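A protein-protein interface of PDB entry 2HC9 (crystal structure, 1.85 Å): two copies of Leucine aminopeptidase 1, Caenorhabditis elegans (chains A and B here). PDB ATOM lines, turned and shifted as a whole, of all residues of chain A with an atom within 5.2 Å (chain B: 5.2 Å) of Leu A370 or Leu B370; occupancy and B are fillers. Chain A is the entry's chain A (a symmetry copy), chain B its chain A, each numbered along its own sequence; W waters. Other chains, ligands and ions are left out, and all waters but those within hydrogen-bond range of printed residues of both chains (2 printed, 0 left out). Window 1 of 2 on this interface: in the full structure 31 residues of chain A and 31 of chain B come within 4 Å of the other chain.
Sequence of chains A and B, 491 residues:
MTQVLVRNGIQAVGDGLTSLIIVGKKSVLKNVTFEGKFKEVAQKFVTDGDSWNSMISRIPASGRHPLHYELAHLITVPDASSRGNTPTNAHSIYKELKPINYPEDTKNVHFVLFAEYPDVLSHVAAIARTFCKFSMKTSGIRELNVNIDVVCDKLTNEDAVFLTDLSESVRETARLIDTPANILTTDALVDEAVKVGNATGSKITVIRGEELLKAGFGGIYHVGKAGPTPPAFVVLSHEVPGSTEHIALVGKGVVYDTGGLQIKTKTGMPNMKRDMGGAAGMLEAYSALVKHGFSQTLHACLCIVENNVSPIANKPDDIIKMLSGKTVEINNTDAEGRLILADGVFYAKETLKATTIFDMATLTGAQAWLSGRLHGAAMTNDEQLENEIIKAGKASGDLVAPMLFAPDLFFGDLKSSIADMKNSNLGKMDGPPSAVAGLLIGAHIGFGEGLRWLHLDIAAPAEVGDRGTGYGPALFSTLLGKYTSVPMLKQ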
ATOM      1  N   ALA A 366     -15.154  23.482  25.337  1.00  0.00           N
ATOM      2  CA  ALA A 366     -15.369  22.156  24.736  1.00  0.00           C
ATOM      3  C   ALA A 366     -15.037  20.998  25.676  1.00  0.00           C
ATOM      4  O   ALA A 366     -15.588  19.901  25.524  1.00  0.00           O
ATOM      5  CB  ALA A 366     -14.569  22.025  23.466  1.00  0.00           C
ATOM      6  N   GLN A 367     -14.147  21.235  26.648  1.00  0.00           N
ATOM      7  CA  GLN A 367     -13.737  20.165  27.585  1.00  0.00           C
ATOM      8  C   GLN A 367     -14.935  19.469  28.283  1.00  0.00           C
ATOM      9  O   GLN A 367     -14.939  18.255  28.415  1.00  0.00           O
ATOM     10  CB  GLN A 367     -12.658  20.694  28.567  1.00  0.00           C
ATOM     11  CG  GLN A 367     -12.347  19.770  29.771  1.00  0.00           C
ATOM     12  CD  GLN A 367     -13.358  19.961  30.898  1.00  0.00           C
ATOM     13  OE1 GLN A 367     -13.612  21.091  31.334  1.00  0.00           O
ATOM     14  NE2 GLN A 367     -13.962  18.867  31.346  1.00  0.00           N
ATOM     15  N   ALA A 368     -15.949  20.243  28.697  1.00  0.00           N
ATOM     16  CA  ALA A 368     -17.152  19.703  29.357  1.00  0.00           C
ATOM     17  C   ALA A 368     -17.914  18.716  28.443  1.00  0.00           C
ATOM     18  O   ALA A 368     -18.590  17.799  28.928  1.00  0.00           O
ATOM     19  CB  ALA A 368     -18.071  20.838  29.785  1.00  0.00           C
ATOM     20  N   TRP A 369     -17.819  18.920  27.124  1.00  0.00           N
ATOM     21  CA  TRP A 369     -18.493  18.002  26.176  1.00  0.00           C
ATOM     22  C   TRP A 369     -17.712  16.692  25.986  1.00  0.00           C
ATOM     23  O   TRP A 369     -18.233  15.707  25.456  1.00  0.00           O
ATOM     24  CB  TRP A 369     -18.750  18.701  24.827  1.00  0.00           C
ATOM     25  CG  TRP A 369     -19.698  19.880  24.947  1.00  0.00           C
ATOM     26  CD1 TRP A 369     -19.548  20.991  25.756  1.00  0.00           C
ATOM     27  CD2 TRP A 369     -20.920  20.075  24.233  1.00  0.00           C
ATOM     28  NE1 TRP A 369     -20.613  21.843  25.589  1.00  0.00           N
ATOM     29  CE2 TRP A 369     -21.470  21.302  24.664  1.00  0.00           C
ATOM     30  CE3 TRP A 369     -21.599  19.338  23.276  1.00  0.00           C
ATOM     31  CZ2 TRP A 369     -22.664  21.805  24.151  1.00  0.00           C
ATOM     32  CZ3 TRP A 369     -22.805  19.834  22.777  1.00  0.00           C
ATOM     33  CH2 TRP A 369     -23.322  21.053  23.217  1.00  0.00           C
ATOM     34  N   LEU A 370     -16.456  16.691  26.408  1.00  0.00           N
ATOM     35  CA  LEU A 370     -15.636  15.499  26.328  1.00  0.00           C
ATOM     36  C   LEU A 370     -15.676  14.701  27.638  1.00  0.00           C
ATOM     37  O   LEU A 370     -15.961  13.492  27.637  1.00  0.00           O
ATOM     38  CB  LEU A 370     -14.204  15.874  25.930  1.00  0.00           C
ATOM     39  CG  LEU A 370     -13.257  14.725  25.533  1.00  0.00           C
ATOM     40  CD1 LEU A 370     -12.153  15.276  24.598  1.00  0.00           C
ATOM     41  CD2 LEU A 370     -12.609  14.106  26.795  1.00  0.00           C
ATOM     42  N   SER A 371     -15.363  15.366  28.758  1.00  0.00           N
ATOM     43  CA  SER A 371     -15.198  14.670  30.039  1.00  0.00           C
ATOM     44  C   SER A 371     -16.193  15.111  31.108  1.00  0.00           C
ATOM     45  O   SER A 371     -16.137  14.628  32.239  1.00  0.00           O
ATOM     46  CB  SER A 371     -13.755  14.830  30.557  1.00  0.00           C
ATOM     47  OG  SER A 371     -13.444  16.185  30.872  1.00  0.00           O
ATOM     48  N   GLY A 372     -17.115  16.011  30.758  1.00  0.00           N
ATOM     49  CA  GLY A 372     -18.101  16.474  31.734  1.00  0.00           C
ATOM     50  C   GLY A 372     -17.488  17.468  32.721  1.00  0.00           C
ATOM     51  O   GLY A 372     -16.399  18.006  32.483  1.00  0.00           O
ATOM     52  N   ALA A 377      -9.659  16.633  31.604  1.00  0.00           N
ATOM     53  CA  ALA A 377      -9.444  15.847  30.392  1.00  0.00           C
ATOM     54  C   ALA A 377      -7.959  15.803  30.108  1.00  0.00           C
ATOM     55  O   ALA A 377      -7.337  16.841  29.889  1.00  0.00           O
ATOM     56  CB  ALA A 377     -10.241  16.499  29.202  1.00  0.00           C
ATOM     57  N   PRO A 402      -9.513  10.320  30.055  1.00  0.00           N
ATOM     58  CA  PRO A 402      -8.569  10.457  28.964  1.00  0.00           C
ATOM     59  C   PRO A 402      -9.159  11.088  27.704  1.00  0.00           C
ATOM     60  O   PRO A 402     -10.338  10.893  27.386  1.00  0.00           O
ATOM     61  CB  PRO A 402      -8.182   8.988  28.661  1.00  0.00           C
ATOM     62  CG  PRO A 402      -9.355   8.210  29.026  1.00  0.00           C
ATOM     63  CD  PRO A 402     -10.083   8.956  30.122  1.00  0.00           C
ATOM     64  N   MET A 403      -8.329  11.888  27.037  1.00  0.00           N
ATOM     65  CA  MET A 403      -8.550  12.360  25.660  1.00  0.00           C
ATOM     66  C   MET A 403      -7.789  11.470  24.695  1.00  0.00           C
ATOM     67  O   MET A 403      -6.778  10.859  25.054  1.00  0.00           O
ATOM     68  CB  MET A 403      -8.021  13.797  25.482  1.00  0.00           C
ATOM     69  CG  MET A 403      -8.837  14.863  26.172  1.00  0.00           C
ATOM     70  SD  MET A 403      -8.860  16.489  25.364  1.00  0.00           S
ATOM     71  CE  MET A 403      -7.578  17.295  26.337  1.00  0.00           C
ATOM     72  N   PRO A 432     -11.509  16.080  18.496  1.00  0.00           N
ATOM     73  CA  PRO A 432     -12.267  16.776  19.566  1.00  0.00           C
ATOM     74  C   PRO A 432     -11.591  18.155  19.763  1.00  0.00           C
ATOM     75  O   PRO A 432     -10.366  18.211  19.816  1.00  0.00           O
ATOM     76  CB  PRO A 432     -12.013  15.900  20.814  1.00  0.00           C
ATOM     77  CG  PRO A 432     -11.382  14.619  20.328  1.00  0.00           C
ATOM     78  CD  PRO A 432     -10.834  14.843  18.952  1.00  0.00           C
ATOM     79  N   SER A 434     -11.075  20.066  22.247  1.00  0.00           N
ATOM     80  CA  SER A 434     -10.166  20.092  23.415  1.00  0.00           C
ATOM     81  C   SER A 434      -8.828  19.405  23.150  1.00  0.00           C
ATOM     82  O   SER A 434      -7.795  19.807  23.699  1.00  0.00           O
ATOM     83  CB  SER A 434     -10.825  19.494  24.655  1.00  0.00           C
ATOM     84  OG  SER A 434     -12.042  20.181  24.914  1.00  0.00           O
ATOM     85  N   ALA A 435      -8.846  18.380  22.299  1.00  0.00           N
ATOM     86  CA  ALA A 435      -7.631  17.658  21.934  1.00  0.00           C
ATOM     87  C   ALA A 435      -6.800  18.518  20.992  1.00  0.00           C
ATOM     88  O   ALA A 435      -5.579  18.631  21.145  1.00  0.00           O
ATOM     89  CB  ALA A 435      -8.009  16.327  21.244  1.00  0.00           C
ATOM     90  N   ALA B 366     -23.006  16.284  19.691  1.00  0.00           N
ATOM     91  CA  ALA B 366     -21.995  16.377  20.756  1.00  0.00           C
ATOM     92  C   ALA B 366     -20.897  15.320  20.651  1.00  0.00           C
ATOM     93  O   ALA B 366     -19.780  15.540  21.134  1.00  0.00           O
ATOM     94  CB  ALA B 366     -22.656  16.292  22.108  1.00  0.00           C
ATOM     95  N   GLN B 367     -21.203  14.180  20.020  1.00  0.00           N
ATOM     96  CA  GLN B 367     -20.216  13.084  19.899  1.00  0.00           C
ATOM     97  C   GLN B 367     -18.864  13.542  19.290  1.00  0.00           C
ATOM     98  O   GLN B 367     -17.816  13.138  19.769  1.00  0.00           O
ATOM     99  CB  GLN B 367     -20.848  11.865  19.177  1.00  0.00           C
ATOM    100  CG  GLN B 367     -19.853  10.764  18.736  1.00  0.00           C
ATOM    101  CD  GLN B 367     -19.189  11.110  17.407  1.00  0.00           C
ATOM    102  OE1 GLN B 367     -19.870  11.430  16.425  1.00  0.00           O
ATOM    103  NE2 GLN B 367     -17.861  11.085  17.381  1.00  0.00           N
ATOM    104  N   ALA B 368     -18.904  14.400  18.261  1.00  0.00           N
ATOM    105  CA  ALA B 368     -17.691  14.925  17.607  1.00  0.00           C
ATOM    106  C   ALA B 368     -16.805  15.720  18.594  1.00  0.00           C
ATOM    107  O   ALA B 368     -15.579  15.785  18.430  1.00  0.00           O
ATOM    108  CB  ALA B 368     -18.070  15.801  16.422  1.00  0.00           C
ATOM    109  N   TRP B 369     -17.430  16.336  19.604  1.00  0.00           N
ATOM    110  CA  TRP B 369     -16.652  17.094  20.613  1.00  0.00           C
ATOM    111  C   TRP B 369     -15.989  16.168  21.645  1.00  0.00           C
ATOM    112  O   TRP B 369     -15.096  16.577  22.392  1.00  0.00           O
ATOM    113  CB  TRP B 369     -17.533  18.156  21.296  1.00  0.00           C
ATOM    114  CG  TRP B 369     -18.030  19.217  20.333  1.00  0.00           C
ATOM    115  CD1 TRP B 369     -18.768  19.016  19.181  1.00  0.00           C
ATOM    116  CD2 TRP B 369     -17.847  20.630  20.441  1.00  0.00           C
ATOM    117  NE1 TRP B 369     -19.030  20.220  18.573  1.00  0.00           N
ATOM    118  CE2 TRP B 369     -18.472  21.225  19.323  1.00  0.00           C
ATOM    119  CE3 TRP B 369     -17.219  21.446  21.367  1.00  0.00           C
ATOM    120  CZ2 TRP B 369     -18.494  22.604  19.126  1.00  0.00           C
ATOM    121  CZ3 TRP B 369     -17.224  22.827  21.159  1.00  0.00           C
ATOM    122  CH2 TRP B 369     -17.857  23.387  20.048  1.00  0.00           C
ATOM    123  N   LEU B 370     -16.440  14.922  21.693  1.00  0.00           N
ATOM    124  CA  LEU B 370     -15.860  13.945  22.590  1.00  0.00           C
ATOM    125  C   LEU B 370     -14.772  13.119  21.893  1.00  0.00           C
ATOM    126  O   LEU B 370     -13.638  13.014  22.389  1.00  0.00           O
ATOM    127  CB  LEU B 370     -16.961  13.058  23.181  1.00  0.00           C
ATOM    128  CG  LEU B 370     -16.574  12.140  24.358  1.00  0.00           C
ATOM    129  CD1 LEU B 370     -17.835  11.834  25.201  1.00  0.00           C
ATOM    130  CD2 LEU B 370     -15.968  10.818  23.827  1.00  0.00           C
ATOM    131  N   SER B 371     -15.117  12.506  20.753  1.00  0.00           N
ATOM    132  CA  SER B 371     -14.218  11.553  20.094  1.00  0.00           C
ATOM    133  C   SER B 371     -13.787  11.985  18.695  1.00  0.00           C
ATOM    134  O   SER B 371     -13.060  11.255  18.022  1.00  0.00           O
ATOM    135  CB  SER B 371     -14.861  10.153  20.044  1.00  0.00           C
ATOM    136  OG  SER B 371     -16.029  10.126  19.227  1.00  0.00           O
ATOM    137  N   GLY B 372     -14.213  13.173  18.259  1.00  0.00           N
ATOM    138  CA  GLY B 372     -13.832  13.649  16.928  1.00  0.00           C
ATOM    139  C   GLY B 372     -14.633  12.945  15.832  1.00  0.00           C
ATOM    140  O   GLY B 372     -15.660  12.310  16.107  1.00  0.00           O
ATOM    141  N   ALA B 377     -17.932   6.764  19.594  1.00  0.00           N
ATOM    142  CA  ALA B 377     -17.760   6.950  21.033  1.00  0.00           C
ATOM    143  C   ALA B 377     -18.503   5.845  21.750  1.00  0.00           C
ATOM    144  O   ALA B 377     -19.720   5.729  21.621  1.00  0.00           O
ATOM    145  CB  ALA B 377     -18.300   8.369  21.442  1.00  0.00           C
ATOM    146  N   PRO B 402     -13.255   5.606  23.960  1.00  0.00           N
ATOM    147  CA  PRO B 402     -14.148   5.391  25.080  1.00  0.00           C
ATOM    148  C   PRO B 402     -14.790   6.667  25.621  1.00  0.00           C
ATOM    149  O   PRO B 402     -14.178   7.742  25.607  1.00  0.00           O
ATOM    150  CB  PRO B 402     -13.206   4.801  26.159  1.00  0.00           C
ATOM    151  CG  PRO B 402     -11.901   5.375  25.871  1.00  0.00           C
ATOM    152  CD  PRO B 402     -11.839   5.660  24.386  1.00  0.00           C
ATOM    153  N   MET B 403     -16.047   6.529  26.039  1.00  0.00           N
ATOM    154  CA  MET B 403     -16.764   7.511  26.867  1.00  0.00           C
ATOM    155  C   MET B 403     -16.683   7.096  28.325  1.00  0.00           C
ATOM    156  O   MET B 403     -16.535   5.912  28.642  1.00  0.00           O
ATOM    157  CB  MET B 403     -18.257   7.566  26.483  1.00  0.00           C
ATOM    158  CG  MET B 403     -18.545   8.209  25.149  1.00  0.00           C
ATOM    159  SD  MET B 403     -20.133   9.079  25.016  1.00  0.00           S
ATOM    160  CE  MET B 403     -21.093   7.775  24.230  1.00  0.00           C
ATOM    161  N   PRO B 432     -20.706  14.480  30.003  1.00  0.00           N
ATOM    162  CA  PRO B 432     -20.596  14.786  28.554  1.00  0.00           C
ATOM    163  C   PRO B 432     -21.992  14.522  27.937  1.00  0.00           C
ATOM    164  O   PRO B 432     -22.591  13.497  28.249  1.00  0.00           O
ATOM    165  CB  PRO B 432     -19.599  13.724  28.037  1.00  0.00           C
ATOM    166  CG  PRO B 432     -18.984  13.075  29.250  1.00  0.00           C
ATOM    167  CD  PRO B 432     -19.853  13.349  30.438  1.00  0.00           C
ATOM    168  N   SER B 434     -23.039  13.433  25.143  1.00  0.00           N
ATOM    169  CA  SER B 434     -23.119  12.123  24.460  1.00  0.00           C
ATOM    170  C   SER B 434     -23.255  10.948  25.426  1.00  0.00           C
ATOM    171  O   SER B 434     -23.897   9.940  25.106  1.00  0.00           O
ATOM    172  CB  SER B 434     -21.929  11.900  23.529  1.00  0.00           C
ATOM    173  OG  SER B 434     -21.852  12.977  22.605  1.00  0.00           O
ATOM    174  N   ALA B 435     -22.663  11.084  26.612  1.00  0.00           N
ATOM    175  CA  ALA B 435     -22.744  10.050  27.638  1.00  0.00           C
ATOM    176  C   ALA B 435     -24.137  10.061  28.254  1.00  0.00           C
ATOM    177  O   ALA B 435     -24.751   9.008  28.455  1.00  0.00           O
ATOM    178  CB  ALA B 435     -21.681  10.321  28.728  1.00  0.00           C
HETATM  179  O   HOH W   1     -13.527  18.679  23.013  1.00  0.00           O
HETATM  180  O   HOH W   2     -20.511  14.702  24.422  1.00  0.00           O
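Water W1 lies within hydrogen-bond range of O of Trp B369, OG of Ser A434 and O of Ala A366.
Water W2 lies within hydrogen-bond range of the backbone carbonyl oxygen (O) of Trp A369 (2.7 Å), the side-chain hydroxyl (OG) of Ser B434 (2.8 Å) and the backbone carbonyl oxygen (O) of Ala B366 (3.5 Å).
Ala A368 touches Pro B432, and with the chains exchanged Pro A432 touches Ala B368.
Trp A369 touches Pro B432, and with the chains exchanged Pro A432 touches Trp B369.
Leu A370 touches its own counterpart, Leu B370.
Leu A370 touches Pro B432, and with the chains exchanged Pro A432 touches Leu B370.
Of the 16 pairs that touch across the chains among the printed residues, 16 have their exchanged pair printed and touching as well.
Hydrophobic or aromatic side chains of chain A that line the printed part of chain B: Ala A366, Trp A369, Leu A370 and Pro A432.
Along chain A the printed residues that touch a printed residue of chain B span positions 366 to 432.
Of the 13 printed residues of chain B, 7 touch a printed residue of chain A.
Hydrophobic or aromatic side chains of chain B that line the printed part of chain A: Ala B366, Trp B369, Leu B370 and Pro B432.
Of the printed residues of chain B, Leu A370 touches Trp B369, Leu B370 and Pro B432.
Printed residues of chain B within 4 Å of Ser A371: Pro B432.
Of the printed residues of chain A, Ala B366 touches Trp A369 (3.4 Å).
Of the printed residues of chain A, Ala B368 touches Pro A432.
Leu B370 touches three residues of chain A.
The nearest printed residue of chain B that does not touch Leu A370 is Ser B371 (5.6 Å).
The nearest printed residue of chain A that does not touch Leu B370 is Ser A371 (5.6 Å).
The nearest printed residue of chain A that does not touch Ala B368 is Trp A369 (7.0 Å).
Among the printed residues, merely in contact across the chains: Trp A369 with Ala B366 (3.4 Å), Ala A366 with Trp B369 (3.4 Å), Pro A432 with Leu B370 (3.5 Å), Leu A370 with Pro B432 (3.5 Å), Leu A370 with Leu B370 (3.5 Å), Pro A432 with Trp B369 (3.5 Å), Trp A369 with Pro B432 (3.5 Å), Pro A432 with Ala B368 (3.6 Å), Ala A368 with Pro B432 (3.6 Å), Gly A372 with Pro B432 (3.7 Å), Pro A432 with Gly B372 (3.7 Å), Leu A370 with Trp B369 (3.7 Å), Trp A369 with Leu B370 (3.7 Å), Trp A369 with Trp B369 (3.8 Å), Ser A371 with Pro B432 (3.9 Å) and Pro A432 with Ser B371 (3.9 Å).
NE2 of Gln B367 lies within hydrogen-bond range of OG of Ser B371 (2.8 Å).
O of Gly B372 is in hydrogen-bond range of NE2 of Gln B367, at 2.8 Å.
OG of Ser A371 sits at hydrogen-bond distance from NE2 of Gln A367 (2.8 Å).
The side-chain amide nitrogen (NE2) of Gln A367 sits at hydrogen-bond distance from the backbone carbonyl oxygen (O) of Gly A372 (2.8 Å).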
